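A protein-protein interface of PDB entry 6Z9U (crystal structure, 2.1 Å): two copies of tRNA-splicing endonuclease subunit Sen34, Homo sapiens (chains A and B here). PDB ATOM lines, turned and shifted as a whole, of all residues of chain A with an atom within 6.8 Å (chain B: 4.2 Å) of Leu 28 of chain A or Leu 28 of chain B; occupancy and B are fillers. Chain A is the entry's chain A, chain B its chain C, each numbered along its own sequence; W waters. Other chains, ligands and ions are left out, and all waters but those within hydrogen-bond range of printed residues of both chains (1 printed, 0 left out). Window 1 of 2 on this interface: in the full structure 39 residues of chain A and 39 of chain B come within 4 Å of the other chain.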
ATOM      1  N   TYR A  15     -13.255 -25.253 -11.577  1.00  0.00           N
ATOM      2  CA  TYR A  15     -12.410 -26.051 -12.454  1.00  0.00           C
ATOM      3  C   TYR A  15     -13.048 -27.385 -12.796  1.00  0.00           C
ATOM      4  O   TYR A  15     -12.763 -27.935 -13.864  1.00  0.00           O
ATOM      5  CB  TYR A  15     -11.012 -26.229 -11.855  1.00  0.00           C
ATOM      6  CG  TYR A  15     -10.076 -25.245 -12.509  1.00  0.00           C
ATOM      7  CD1 TYR A  15      -9.999 -23.935 -12.056  1.00  0.00           C
ATOM      8  CD2 TYR A  15      -9.320 -25.604 -13.633  1.00  0.00           C
ATOM      9  CE1 TYR A  15      -9.174 -23.014 -12.675  1.00  0.00           C
ATOM     10  CE2 TYR A  15      -8.494 -24.689 -14.258  1.00  0.00           C
ATOM     11  CZ  TYR A  15      -8.430 -23.392 -13.771  1.00  0.00           C
ATOM     12  OH  TYR A  15      -7.620 -22.457 -14.370  1.00  0.00           O
ATOM     13  N   ILE A  17     -16.000 -27.596 -13.732  1.00  0.00           N
ATOM     14  CA  ILE A  17     -16.782 -27.269 -14.918  1.00  0.00           C
ATOM     15  C   ILE A  17     -15.876 -27.010 -16.112  1.00  0.00           C
ATOM     16  O   ILE A  17     -16.134 -27.501 -17.221  1.00  0.00           O
ATOM     17  CB  ILE A  17     -17.705 -26.078 -14.622  1.00  0.00           C
ATOM     18  CG1 ILE A  17     -18.811 -26.554 -13.684  1.00  0.00           C
ATOM     19  CG2 ILE A  17     -18.266 -25.493 -15.914  1.00  0.00           C
ATOM     20  CD1 ILE A  17     -19.612 -25.473 -13.102  1.00  0.00           C
ATOM     21  N   TYR A  18     -14.804 -26.244 -15.903  1.00  0.00           N
ATOM     22  CA  TYR A  18     -13.818 -26.029 -16.962  1.00  0.00           C
ATOM     23  C   TYR A  18     -13.385 -27.342 -17.604  1.00  0.00           C
ATOM     24  O   TYR A  18     -13.423 -27.487 -18.830  1.00  0.00           O
ATOM     25  CB  TYR A  18     -12.601 -25.290 -16.398  1.00  0.00           C
ATOM     26  CG  TYR A  18     -12.926 -23.918 -15.873  1.00  0.00           C
ATOM     27  CD1 TYR A  18     -12.041 -23.253 -15.039  1.00  0.00           C
ATOM     28  CD2 TYR A  18     -14.131 -23.282 -16.208  1.00  0.00           C
ATOM     29  CE1 TYR A  18     -12.332 -21.987 -14.553  1.00  0.00           C
ATOM     30  CE2 TYR A  18     -14.431 -22.024 -15.728  1.00  0.00           C
ATOM     31  CZ  TYR A  18     -13.519 -21.374 -14.902  1.00  0.00           C
ATOM     32  OH  TYR A  18     -13.779 -20.112 -14.407  1.00  0.00           O
ATOM     33  N   ARG A  19     -12.991 -28.325 -16.787  1.00  0.00           N
ATOM     34  CA  ARG A  19     -12.475 -29.566 -17.352  1.00  0.00           C
ATOM     35  C   ARG A  19     -13.548 -30.301 -18.135  1.00  0.00           C
ATOM     36  O   ARG A  19     -13.248 -30.941 -19.157  1.00  0.00           O
ATOM     37  CB  ARG A  19     -11.890 -30.470 -16.262  1.00  0.00           C
ATOM     38  CG  ARG A  19     -10.863 -29.787 -15.367  1.00  0.00           C
ATOM     39  CD  ARG A  19      -9.981 -30.803 -14.633  1.00  0.00           C
ATOM     40  NE  ARG A  19      -9.837 -30.466 -13.223  1.00  0.00           N
ATOM     41  CZ  ARG A  19     -10.619 -30.956 -12.265  1.00  0.00           C
ATOM     42  NH1 ARG A  19     -11.586 -31.812 -12.572  1.00  0.00           N
ATOM     43  NH2 ARG A  19     -10.434 -30.596 -11.000  1.00  0.00           N
ATOM     44  N   LEU A  21     -16.110 -28.851 -19.741  1.00  0.00           N
ATOM     45  CA  LEU A  21     -16.227 -28.125 -20.999  1.00  0.00           C
ATOM     46  C   LEU A  21     -15.020 -28.377 -21.890  1.00  0.00           C
ATOM     47  O   LEU A  21     -15.161 -28.552 -23.107  1.00  0.00           O
ATOM     48  CB  LEU A  21     -16.402 -26.639 -20.714  1.00  0.00           C
ATOM     49  CG  LEU A  21     -17.769 -26.388 -20.055  1.00  0.00           C
ATOM     50  CD1 LEU A  21     -17.877 -24.961 -19.618  1.00  0.00           C
ATOM     51  CD2 LEU A  21     -18.835 -26.710 -21.059  1.00  0.00           C
ATOM     52  N   TRP A  22     -13.824 -28.416 -21.307  1.00  0.00           N
ATOM     53  CA  TRP A  22     -12.663 -28.787 -22.109  1.00  0.00           C
ATOM     54  C   TRP A  22     -12.842 -30.174 -22.704  1.00  0.00           C
ATOM     55  O   TRP A  22     -12.648 -30.366 -23.912  1.00  0.00           O
ATOM     56  CB  TRP A  22     -11.383 -28.662 -21.269  1.00  0.00           C
ATOM     57  CG  TRP A  22     -10.942 -27.198 -21.187  1.00  0.00           C
ATOM     58  CD1 TRP A  22     -11.099 -26.246 -22.167  1.00  0.00           C
ATOM     59  CD2 TRP A  22     -10.321 -26.529 -20.075  1.00  0.00           C
ATOM     60  NE1 TRP A  22     -10.605 -25.033 -21.735  1.00  0.00           N
ATOM     61  CE2 TRP A  22     -10.116 -25.181 -20.458  1.00  0.00           C
ATOM     62  CE3 TRP A  22      -9.899 -26.939 -18.803  1.00  0.00           C
ATOM     63  CZ2 TRP A  22      -9.520 -24.244 -19.610  1.00  0.00           C
ATOM     64  CZ3 TRP A  22      -9.294 -26.007 -17.966  1.00  0.00           C
ATOM     65  CH2 TRP A  22      -9.111 -24.676 -18.376  1.00  0.00           C
ATOM     66  N   PHE A  26     -14.868 -27.484 -25.932  1.00  0.00           N
ATOM     67  CA  PHE A  26     -15.072 -26.047 -26.033  1.00  0.00           C
ATOM     68  C   PHE A  26     -13.764 -25.285 -25.832  1.00  0.00           C
ATOM     69  O   PHE A  26     -12.827 -25.774 -25.199  1.00  0.00           O
ATOM     70  CB  PHE A  26     -16.102 -25.562 -24.996  1.00  0.00           C
ATOM     71  CG  PHE A  26     -17.507 -26.051 -25.244  1.00  0.00           C
ATOM     72  CD1 PHE A  26     -17.995 -27.173 -24.579  1.00  0.00           C
ATOM     73  CD2 PHE A  26     -18.353 -25.366 -26.113  1.00  0.00           C
ATOM     74  CE1 PHE A  26     -19.311 -27.624 -24.799  1.00  0.00           C
ATOM     75  CE2 PHE A  26     -19.645 -25.809 -26.340  1.00  0.00           C
ATOM     76  CZ  PHE A  26     -20.129 -26.941 -25.683  1.00  0.00           C
ATOM     77  N   PHE A  27     -13.716 -24.069 -26.378  1.00  0.00           N
ATOM     78  CA  PHE A  27     -12.757 -23.063 -25.936  1.00  0.00           C
ATOM     79  C   PHE A  27     -13.317 -22.290 -24.749  1.00  0.00           C
ATOM     80  O   PHE A  27     -14.503 -21.942 -24.728  1.00  0.00           O
ATOM     81  CB  PHE A  27     -12.453 -22.027 -27.022  1.00  0.00           C
ATOM     82  CG  PHE A  27     -12.130 -22.571 -28.353  1.00  0.00           C
ATOM     83  CD1 PHE A  27     -10.793 -22.643 -28.774  1.00  0.00           C
ATOM     84  CD2 PHE A  27     -13.134 -22.928 -29.235  1.00  0.00           C
ATOM     85  CE1 PHE A  27     -10.461 -23.099 -30.029  1.00  0.00           C
ATOM     86  CE2 PHE A  27     -12.810 -23.401 -30.501  1.00  0.00           C
ATOM     87  CZ  PHE A  27     -11.453 -23.487 -30.899  1.00  0.00           C
ATOM     88  N   LEU A  28     -12.435 -21.917 -23.816  1.00  0.00           N
ATOM     89  CA  LEU A  28     -12.812 -21.157 -22.632  1.00  0.00           C
ATOM     90  C   LEU A  28     -11.932 -19.926 -22.444  1.00  0.00           C
ATOM     91  O   LEU A  28     -10.709 -19.983 -22.621  1.00  0.00           O
ATOM     92  CB  LEU A  28     -12.704 -21.997 -21.369  1.00  0.00           C
ATOM     93  CG  LEU A  28     -13.443 -23.319 -21.341  1.00  0.00           C
ATOM     94  CD1 LEU A  28     -13.269 -23.974 -19.977  1.00  0.00           C
ATOM     95  CD2 LEU A  28     -14.898 -23.059 -21.665  1.00  0.00           C
ATOM     96  N   SER A  29     -12.557 -18.825 -22.034  1.00  0.00           N
ATOM     97  CA  SER A  29     -11.853 -17.699 -21.433  1.00  0.00           C
ATOM     98  C   SER A  29     -12.537 -17.333 -20.131  1.00  0.00           C
ATOM     99  O   SER A  29     -13.727 -17.002 -20.134  1.00  0.00           O
ATOM    100  CB  SER A  29     -11.818 -16.483 -22.354  1.00  0.00           C
ATOM    101  OG  SER A  29     -11.354 -15.372 -21.603  1.00  0.00           O
ATOM    102  N   ALA A  30     -11.784 -17.371 -19.036  1.00  0.00           N
ATOM    103  CA  ALA A  30     -12.262 -17.031 -17.702  1.00  0.00           C
ATOM    104  C   ALA A  30     -11.439 -15.897 -17.111  1.00  0.00           C
ATOM    105  O   ALA A  30     -11.041 -15.926 -15.943  1.00  0.00           O
ATOM    106  CB  ALA A  30     -12.231 -18.254 -16.783  1.00  0.00           C
ATOM    107  N   PHE A  38     -17.792 -16.496 -17.412  1.00  0.00           N
ATOM    108  CA  PHE A  38     -16.725 -16.840 -18.343  1.00  0.00           C
ATOM    109  C   PHE A  38     -17.374 -17.171 -19.673  1.00  0.00           C
ATOM    110  O   PHE A  38     -18.576 -17.441 -19.743  1.00  0.00           O
ATOM    111  CB  PHE A  38     -15.854 -17.999 -17.836  1.00  0.00           C
ATOM    112  CG  PHE A  38     -16.623 -19.245 -17.522  1.00  0.00           C
ATOM    113  CD1 PHE A  38     -16.662 -20.300 -18.418  1.00  0.00           C
ATOM    114  CD2 PHE A  38     -17.312 -19.360 -16.329  1.00  0.00           C
ATOM    115  CE1 PHE A  38     -17.366 -21.447 -18.119  1.00  0.00           C
ATOM    116  CE2 PHE A  38     -18.021 -20.495 -16.029  1.00  0.00           C
ATOM    117  CZ  PHE A  38     -18.055 -21.540 -16.921  1.00  0.00           C
ATOM    118  N   LEU A  39     -16.578 -17.132 -20.737  1.00  0.00           N
ATOM    119  CA  LEU A  39     -17.112 -17.296 -22.079  1.00  0.00           C
ATOM    120  C   LEU A  39     -16.807 -18.688 -22.604  1.00  0.00           C
ATOM    121  O   LEU A  39     -15.695 -19.209 -22.428  1.00  0.00           O
ATOM    122  CB  LEU A  39     -16.543 -16.256 -23.037  1.00  0.00           C
ATOM    123  CG  LEU A  39     -16.636 -14.776 -22.714  1.00  0.00           C
ATOM    124  CD1 LEU A  39     -16.496 -13.991 -24.010  1.00  0.00           C
ATOM    125  CD2 LEU A  39     -17.957 -14.454 -22.025  1.00  0.00           C
ATOM    126  N   VAL A  40     -17.789 -19.276 -23.281  1.00  0.00           N
ATOM    127  CA  VAL A  40     -17.689 -20.647 -23.756  1.00  0.00           C
ATOM    128  C   VAL A  40     -18.038 -20.676 -25.235  1.00  0.00           C
ATOM    129  O   VAL A  40     -19.176 -20.372 -25.613  1.00  0.00           O
ATOM    130  CB  VAL A  40     -18.595 -21.592 -22.950  1.00  0.00           C
ATOM    131  CG1 VAL A  40     -18.546 -23.003 -23.515  1.00  0.00           C
ATOM    132  CG2 VAL A  40     -18.139 -21.587 -21.496  1.00  0.00           C
ATOM    133  N   TYR A  41     -17.058 -21.076 -26.074  1.00  0.00           N
ATOM    134  CA  TYR A  41     -17.164 -21.112 -27.536  1.00  0.00           C
ATOM    135  C   TYR A  41     -17.154 -22.553 -28.026  1.00  0.00           C
ATOM    136  O   TYR A  41     -16.287 -23.334 -27.601  1.00  0.00           O
ATOM    137  CB  TYR A  41     -15.993 -20.344 -28.203  1.00  0.00           C
ATOM    138  CG  TYR A  41     -16.025 -18.830 -28.102  1.00  0.00           C
ATOM    139  CD1 TYR A  41     -16.359 -18.047 -29.205  1.00  0.00           C
ATOM    140  CD2 TYR A  41     -15.697 -18.188 -26.916  1.00  0.00           C
ATOM    141  CE1 TYR A  41     -16.396 -16.667 -29.117  1.00  0.00           C
ATOM    142  CE2 TYR A  41     -15.732 -16.805 -26.817  1.00  0.00           C
ATOM    143  CZ  TYR A  41     -16.083 -16.055 -27.917  1.00  0.00           C
ATOM    144  OH  TYR A  41     -16.103 -14.692 -27.813  1.00  0.00           O
ATOM    145  N   ALA A  54       0.926 -25.737 -25.585  1.00  0.00           N
ATOM    146  CA  ALA A  54       1.567 -25.133 -24.429  1.00  0.00           C
ATOM    147  C   ALA A  54       1.894 -26.180 -23.379  1.00  0.00           C
ATOM    148  O   ALA A  54       1.291 -27.252 -23.329  1.00  0.00           O
ATOM    149  CB  ALA A  54       0.678 -24.049 -23.812  1.00  0.00           C
ATOM    150  N   TYR B  18      -2.890 -20.461 -16.578  1.00  0.00           N
ATOM    151  CA  TYR B  18      -4.202 -20.344 -17.217  1.00  0.00           C
ATOM    152  C   TYR B  18      -4.796 -18.956 -17.004  1.00  0.00           C
ATOM    153  O   TYR B  18      -5.367 -18.355 -17.926  1.00  0.00           O
ATOM    154  CB  TYR B  18      -5.175 -21.405 -16.669  1.00  0.00           C
ATOM    155  CG  TYR B  18      -4.921 -22.815 -17.150  1.00  0.00           C
ATOM    156  CD1 TYR B  18      -3.783 -23.127 -17.903  1.00  0.00           C
ATOM    157  CD2 TYR B  18      -5.815 -23.845 -16.850  1.00  0.00           C
ATOM    158  CE1 TYR B  18      -3.552 -24.418 -18.340  1.00  0.00           C
ATOM    159  CE2 TYR B  18      -5.587 -25.145 -17.282  1.00  0.00           C
ATOM    160  CZ  TYR B  18      -4.451 -25.425 -18.031  1.00  0.00           C
ATOM    161  OH  TYR B  18      -4.225 -26.714 -18.468  1.00  0.00           O
ATOM    162  N   LEU B  21      -2.842 -16.336 -19.063  1.00  0.00           N
ATOM    163  CA  LEU B  21      -3.215 -16.440 -20.472  1.00  0.00           C
ATOM    164  C   LEU B  21      -4.614 -15.868 -20.716  1.00  0.00           C
ATOM    165  O   LEU B  21      -4.836 -15.148 -21.702  1.00  0.00           O
ATOM    166  CB  LEU B  21      -3.149 -17.889 -20.931  1.00  0.00           C
ATOM    167  CG  LEU B  21      -1.680 -18.354 -21.159  1.00  0.00           C
ATOM    168  CD1 LEU B  21      -1.643 -19.825 -21.433  1.00  0.00           C
ATOM    169  CD2 LEU B  21      -0.994 -17.586 -22.297  1.00  0.00           C
ATOM    170  N   TRP B  22      -5.568 -16.179 -19.828  1.00  0.00           N
ATOM    171  CA  TRP B  22      -6.887 -15.555 -19.926  1.00  0.00           C
ATOM    172  C   TRP B  22      -6.785 -14.039 -19.860  1.00  0.00           C
ATOM    173  O   TRP B  22      -7.304 -13.344 -20.742  1.00  0.00           O
ATOM    174  CB  TRP B  22      -7.821 -16.091 -18.836  1.00  0.00           C
ATOM    175  CG  TRP B  22      -8.380 -17.435 -19.192  1.00  0.00           C
ATOM    176  CD1 TRP B  22      -8.690 -17.882 -20.440  1.00  0.00           C
ATOM    177  CD2 TRP B  22      -8.619 -18.533 -18.299  1.00  0.00           C
ATOM    178  NE1 TRP B  22      -9.128 -19.185 -20.382  1.00  0.00           N
ATOM    179  CE2 TRP B  22      -9.095 -19.606 -19.078  1.00  0.00           C
ATOM    180  CE3 TRP B  22      -8.495 -18.703 -16.920  1.00  0.00           C
ATOM    181  CZ2 TRP B  22      -9.459 -20.828 -18.522  1.00  0.00           C
ATOM    182  CZ3 TRP B  22      -8.850 -19.923 -16.370  1.00  0.00           C
ATOM    183  CH2 TRP B  22      -9.321 -20.969 -17.171  1.00  0.00           C
ATOM    184  N   PHE B  27      -7.695 -17.762 -25.583  1.00  0.00           N
ATOM    185  CA  PHE B  27      -8.648 -18.823 -25.285  1.00  0.00           C
ATOM    186  C   PHE B  27      -7.910 -20.142 -25.079  1.00  0.00           C
ATOM    187  O   PHE B  27      -6.967 -20.456 -25.822  1.00  0.00           O
ATOM    188  CB  PHE B  27      -9.666 -18.999 -26.422  1.00  0.00           C
ATOM    189  CG  PHE B  27     -10.642 -17.855 -26.573  1.00  0.00           C
ATOM    190  CD1 PHE B  27     -11.538 -17.833 -27.641  1.00  0.00           C
ATOM    191  CD2 PHE B  27     -10.676 -16.813 -25.661  1.00  0.00           C
ATOM    192  CE1 PHE B  27     -12.444 -16.791 -27.793  1.00  0.00           C
ATOM    193  CE2 PHE B  27     -11.582 -15.764 -25.808  1.00  0.00           C
ATOM    194  CZ  PHE B  27     -12.461 -15.754 -26.872  1.00  0.00           C
ATOM    195  N   LEU B  28      -8.359 -20.925 -24.093  1.00  0.00           N
ATOM    196  CA  LEU B  28      -7.782 -22.237 -23.795  1.00  0.00           C
ATOM    197  C   LEU B  28      -8.743 -23.339 -24.212  1.00  0.00           C
ATOM    198  O   LEU B  28      -9.943 -23.280 -23.897  1.00  0.00           O
ATOM    199  CB  LEU B  28      -7.479 -22.375 -22.301  1.00  0.00           C
ATOM    200  CG  LEU B  28      -6.454 -21.371 -21.746  1.00  0.00           C
ATOM    201  CD1 LEU B  28      -5.939 -21.850 -20.417  1.00  0.00           C
ATOM    202  CD2 LEU B  28      -5.322 -21.162 -22.726  1.00  0.00           C
ATOM    203  N   SER B  29      -8.224 -24.336 -24.924  1.00  0.00           N
ATOM    204  CA  SER B  29      -8.944 -25.571 -25.156  1.00  0.00           C
ATOM    205  C   SER B  29      -8.043 -26.739 -24.795  1.00  0.00           C
ATOM    206  O   SER B  29      -6.814 -26.593 -24.678  1.00  0.00           O
ATOM    207  CB  SER B  29      -9.429 -25.716 -26.602  1.00  0.00           C
ATOM    208  OG  SER B  29      -8.348 -25.891 -27.496  1.00  0.00           O
ATOM    209  N   PHE B  38      -1.684 -28.314 -23.315  1.00  0.00           N
ATOM    210  CA  PHE B  38      -2.971 -27.695 -23.555  1.00  0.00           C
ATOM    211  C   PHE B  38      -2.813 -26.784 -24.756  1.00  0.00           C
ATOM    212  O   PHE B  38      -1.702 -26.587 -25.278  1.00  0.00           O
ATOM    213  CB  PHE B  38      -3.496 -26.942 -22.320  1.00  0.00           C
ATOM    214  CG  PHE B  38      -2.584 -25.854 -21.799  1.00  0.00           C
ATOM    215  CD1 PHE B  38      -2.954 -24.518 -21.910  1.00  0.00           C
ATOM    216  CD2 PHE B  38      -1.390 -26.164 -21.153  1.00  0.00           C
ATOM    217  CE1 PHE B  38      -2.144 -23.531 -21.431  1.00  0.00           C
ATOM    218  CE2 PHE B  38      -0.568 -25.171 -20.660  1.00  0.00           C
ATOM    219  CZ  PHE B  38      -0.940 -23.857 -20.798  1.00  0.00           C
ATOM    220  N   LEU B  39      -3.939 -26.262 -25.224  1.00  0.00           N
ATOM    221  CA  LEU B  39      -3.955 -25.469 -26.440  1.00  0.00           C
ATOM    222  C   LEU B  39      -4.236 -24.026 -26.049  1.00  0.00           C
ATOM    223  O   LEU B  39      -4.946 -23.766 -25.073  1.00  0.00           O
ATOM    224  CB  LEU B  39      -4.983 -26.014 -27.430  1.00  0.00           C
ATOM    225  CG  LEU B  39      -4.697 -27.467 -27.793  1.00  0.00           C
ATOM    226  CD1 LEU B  39      -5.489 -27.912 -28.997  1.00  0.00           C
ATOM    227  CD2 LEU B  39      -3.181 -27.649 -28.106  1.00  0.00           C
ATOM    228  N   VAL B  40      -3.623 -23.090 -26.762  1.00  0.00           N
ATOM    229  CA  VAL B  40      -3.742 -21.669 -26.471  1.00  0.00           C
ATOM    230  C   VAL B  40      -4.031 -20.982 -27.784  1.00  0.00           C
ATOM    231  O   VAL B  40      -3.195 -21.017 -28.693  1.00  0.00           O
ATOM    232  CB  VAL B  40      -2.469 -21.083 -25.844  1.00  0.00           C
ATOM    233  CG1 VAL B  40      -2.624 -19.570 -25.678  1.00  0.00           C
ATOM    234  CG2 VAL B  40      -2.158 -21.767 -24.525  1.00  0.00           C
HETATM  235  O   HOH W   1      -9.065 -14.489 -22.503  1.00  0.00           O
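The indole nitrogen (NE1) of Trp 22 of chain B sits close to the backbone NH (N) of Ala 30 of chain A (3.5 Å).
The backbone NH of Ala 54 of chain A sits at hydrogen-bond distance from the backbone carbonyl oxygen of Phe 38 of chain B, at 2.8 Å.
The backbone carbonyl oxygen (O) of Leu 28 of chain B lies within hydrogen-bond range of the indole nitrogen (NE1) of Trp 22 of chain A.
The indole nitrogen (NE1) of Trp 22 of chain B lies within hydrogen-bond range of the backbone carbonyl oxygen (O) of Leu 28 of chain A, 2.9 Å away.
The backbone NH of Leu 28 of chain A sits at hydrogen-bond distance from the backbone carbonyl oxygen of Leu 28 of chain B, at 2.8 Å.
The backbone carbonyl oxygen of Leu 21 of chain A lies within hydrogen-bond range of the backbone NH of Phe 26 of chain A.
The backbone NH (N) of Leu 39 of chain B is in hydrogen-bond range of the backbone carbonyl oxygen (O) of Ser 29 of chain B, at 2.9 Å.
The backbone carbonyl oxygen (O) of Ser 29 of chain A is in hydrogen-bond range of the backbone NH (N) of Leu 39 of chain A (2.9 Å).
The backbone NH of Phe 27 of chain A lies within hydrogen-bond range of the backbone carbonyl oxygen of Tyr 41 of chain A, 2.9 Å away.
CZ3 of Trp 22 of chain B touches OH of Tyr 15 of chain A, 3.5 Å away.
CZ2 of Trp 22 of chain B touches CZ2 of Trp 22 of chain A (3.6 Å).
CD1 of Trp 22 of chain A touches CA of Ser 29 of chain B (3.7 Å).
O of Phe 26 of chain A touches CB of Ser 29 of chain B (3.7 Å).
Phe 27 of chain A touches Leu 28 of chain B.
Leu 28 of chain A touches Phe 27 of chain B (O to CA, 3.6 Å).
Ser 29 of chain A touches Trp 22 of chain B.
CD2 of Phe 27 of chain B touches CB of Ser 29 of chain A, at 3.5 Å.
Tyr 41 of chain A touches Phe 27 of chain B.
Ala 54 of chain A touches Val 40 of chain B (CB to CG2, 3.7 Å).
Leu 28 of chain A touches just these residues of chain B: Trp 22 (2.9 Å), Phe 27 (3.6 Å) and Leu 28 (2.8 Å).
Of chain A, only Trp 22, Phe 27 and Leu 28 come within 4 Å of Leu 28 of chain B.
Of the printed residues of chain B, Ser 29 of chain A touches Trp 22 (3.3 Å) and Phe 27 (3.5 Å).
Printed residues of chain A within 4 Å of Val 40 of chain B: Ala 54.
Printed residues of chain B within 4 Å of Ala 54 of chain A: Phe 38 and Val 40.
Tyr 18 of chain A touches none of the printed residues of chain B.
The nearest printed residue of chain B that does not touch Leu 28 of chain A is Ser 29 of chain B (5.0 Å).
Of the 16 printed residues of chain A, 9 touch a printed residue of chain B.
Printed residues of chain A that touch a printed residue of chain B: Tyr 15, Trp 22, Phe 26, Phe 27, Leu 28, Ser 29, Ala 30, Tyr 41 and Ala 54.
Hydrophobic or aromatic side chains of chain A within 4 Å of the printed part of chain B: Tyr 15, Trp 22, Leu 28, Ala 30, Tyr 41 and Ala 54.
Of the 9 printed residues of chain B, 7 touch a printed residue of chain A.
Along chain B the printed residues that touch a printed residue of chain A span positions 18 to 40.
Among the printed residues, no Asp or Glu carboxylate lies within 4 Å of a Lys or Arg side-chain nitrogen of the other chain.
Trp 22 of chain A touches its own counterpart, Trp 22 of chain B.
Trp 22 of chain A touches Ser 29 of chain B, and with the chains exchanged Ser 29 of chain A touches Trp 22 of chain B.
Phe 27 of chain A touches Leu 28 of chain B, and with the chains exchanged Leu 28 of chain A touches Phe 27 of chain B.
Ser 29 of chain A touches Phe 27 of chain B, but with the chains exchanged Phe 27 of chain A does not touch Ser 29 of chain B (4.003 Å).
Positions printed for both chains: 18, 21, 22, 27, 28, 29, 38, 39 and 40.
Of the 17 pairs that touch across the chains among the printed residues, 8 have their exchanged pair printed and touching as well.
Water W1 lies within hydrogen-bond range of OG of Ser 29 of chain A (2.6 Å) and O of Trp 22 of chain B (2.7 Å).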
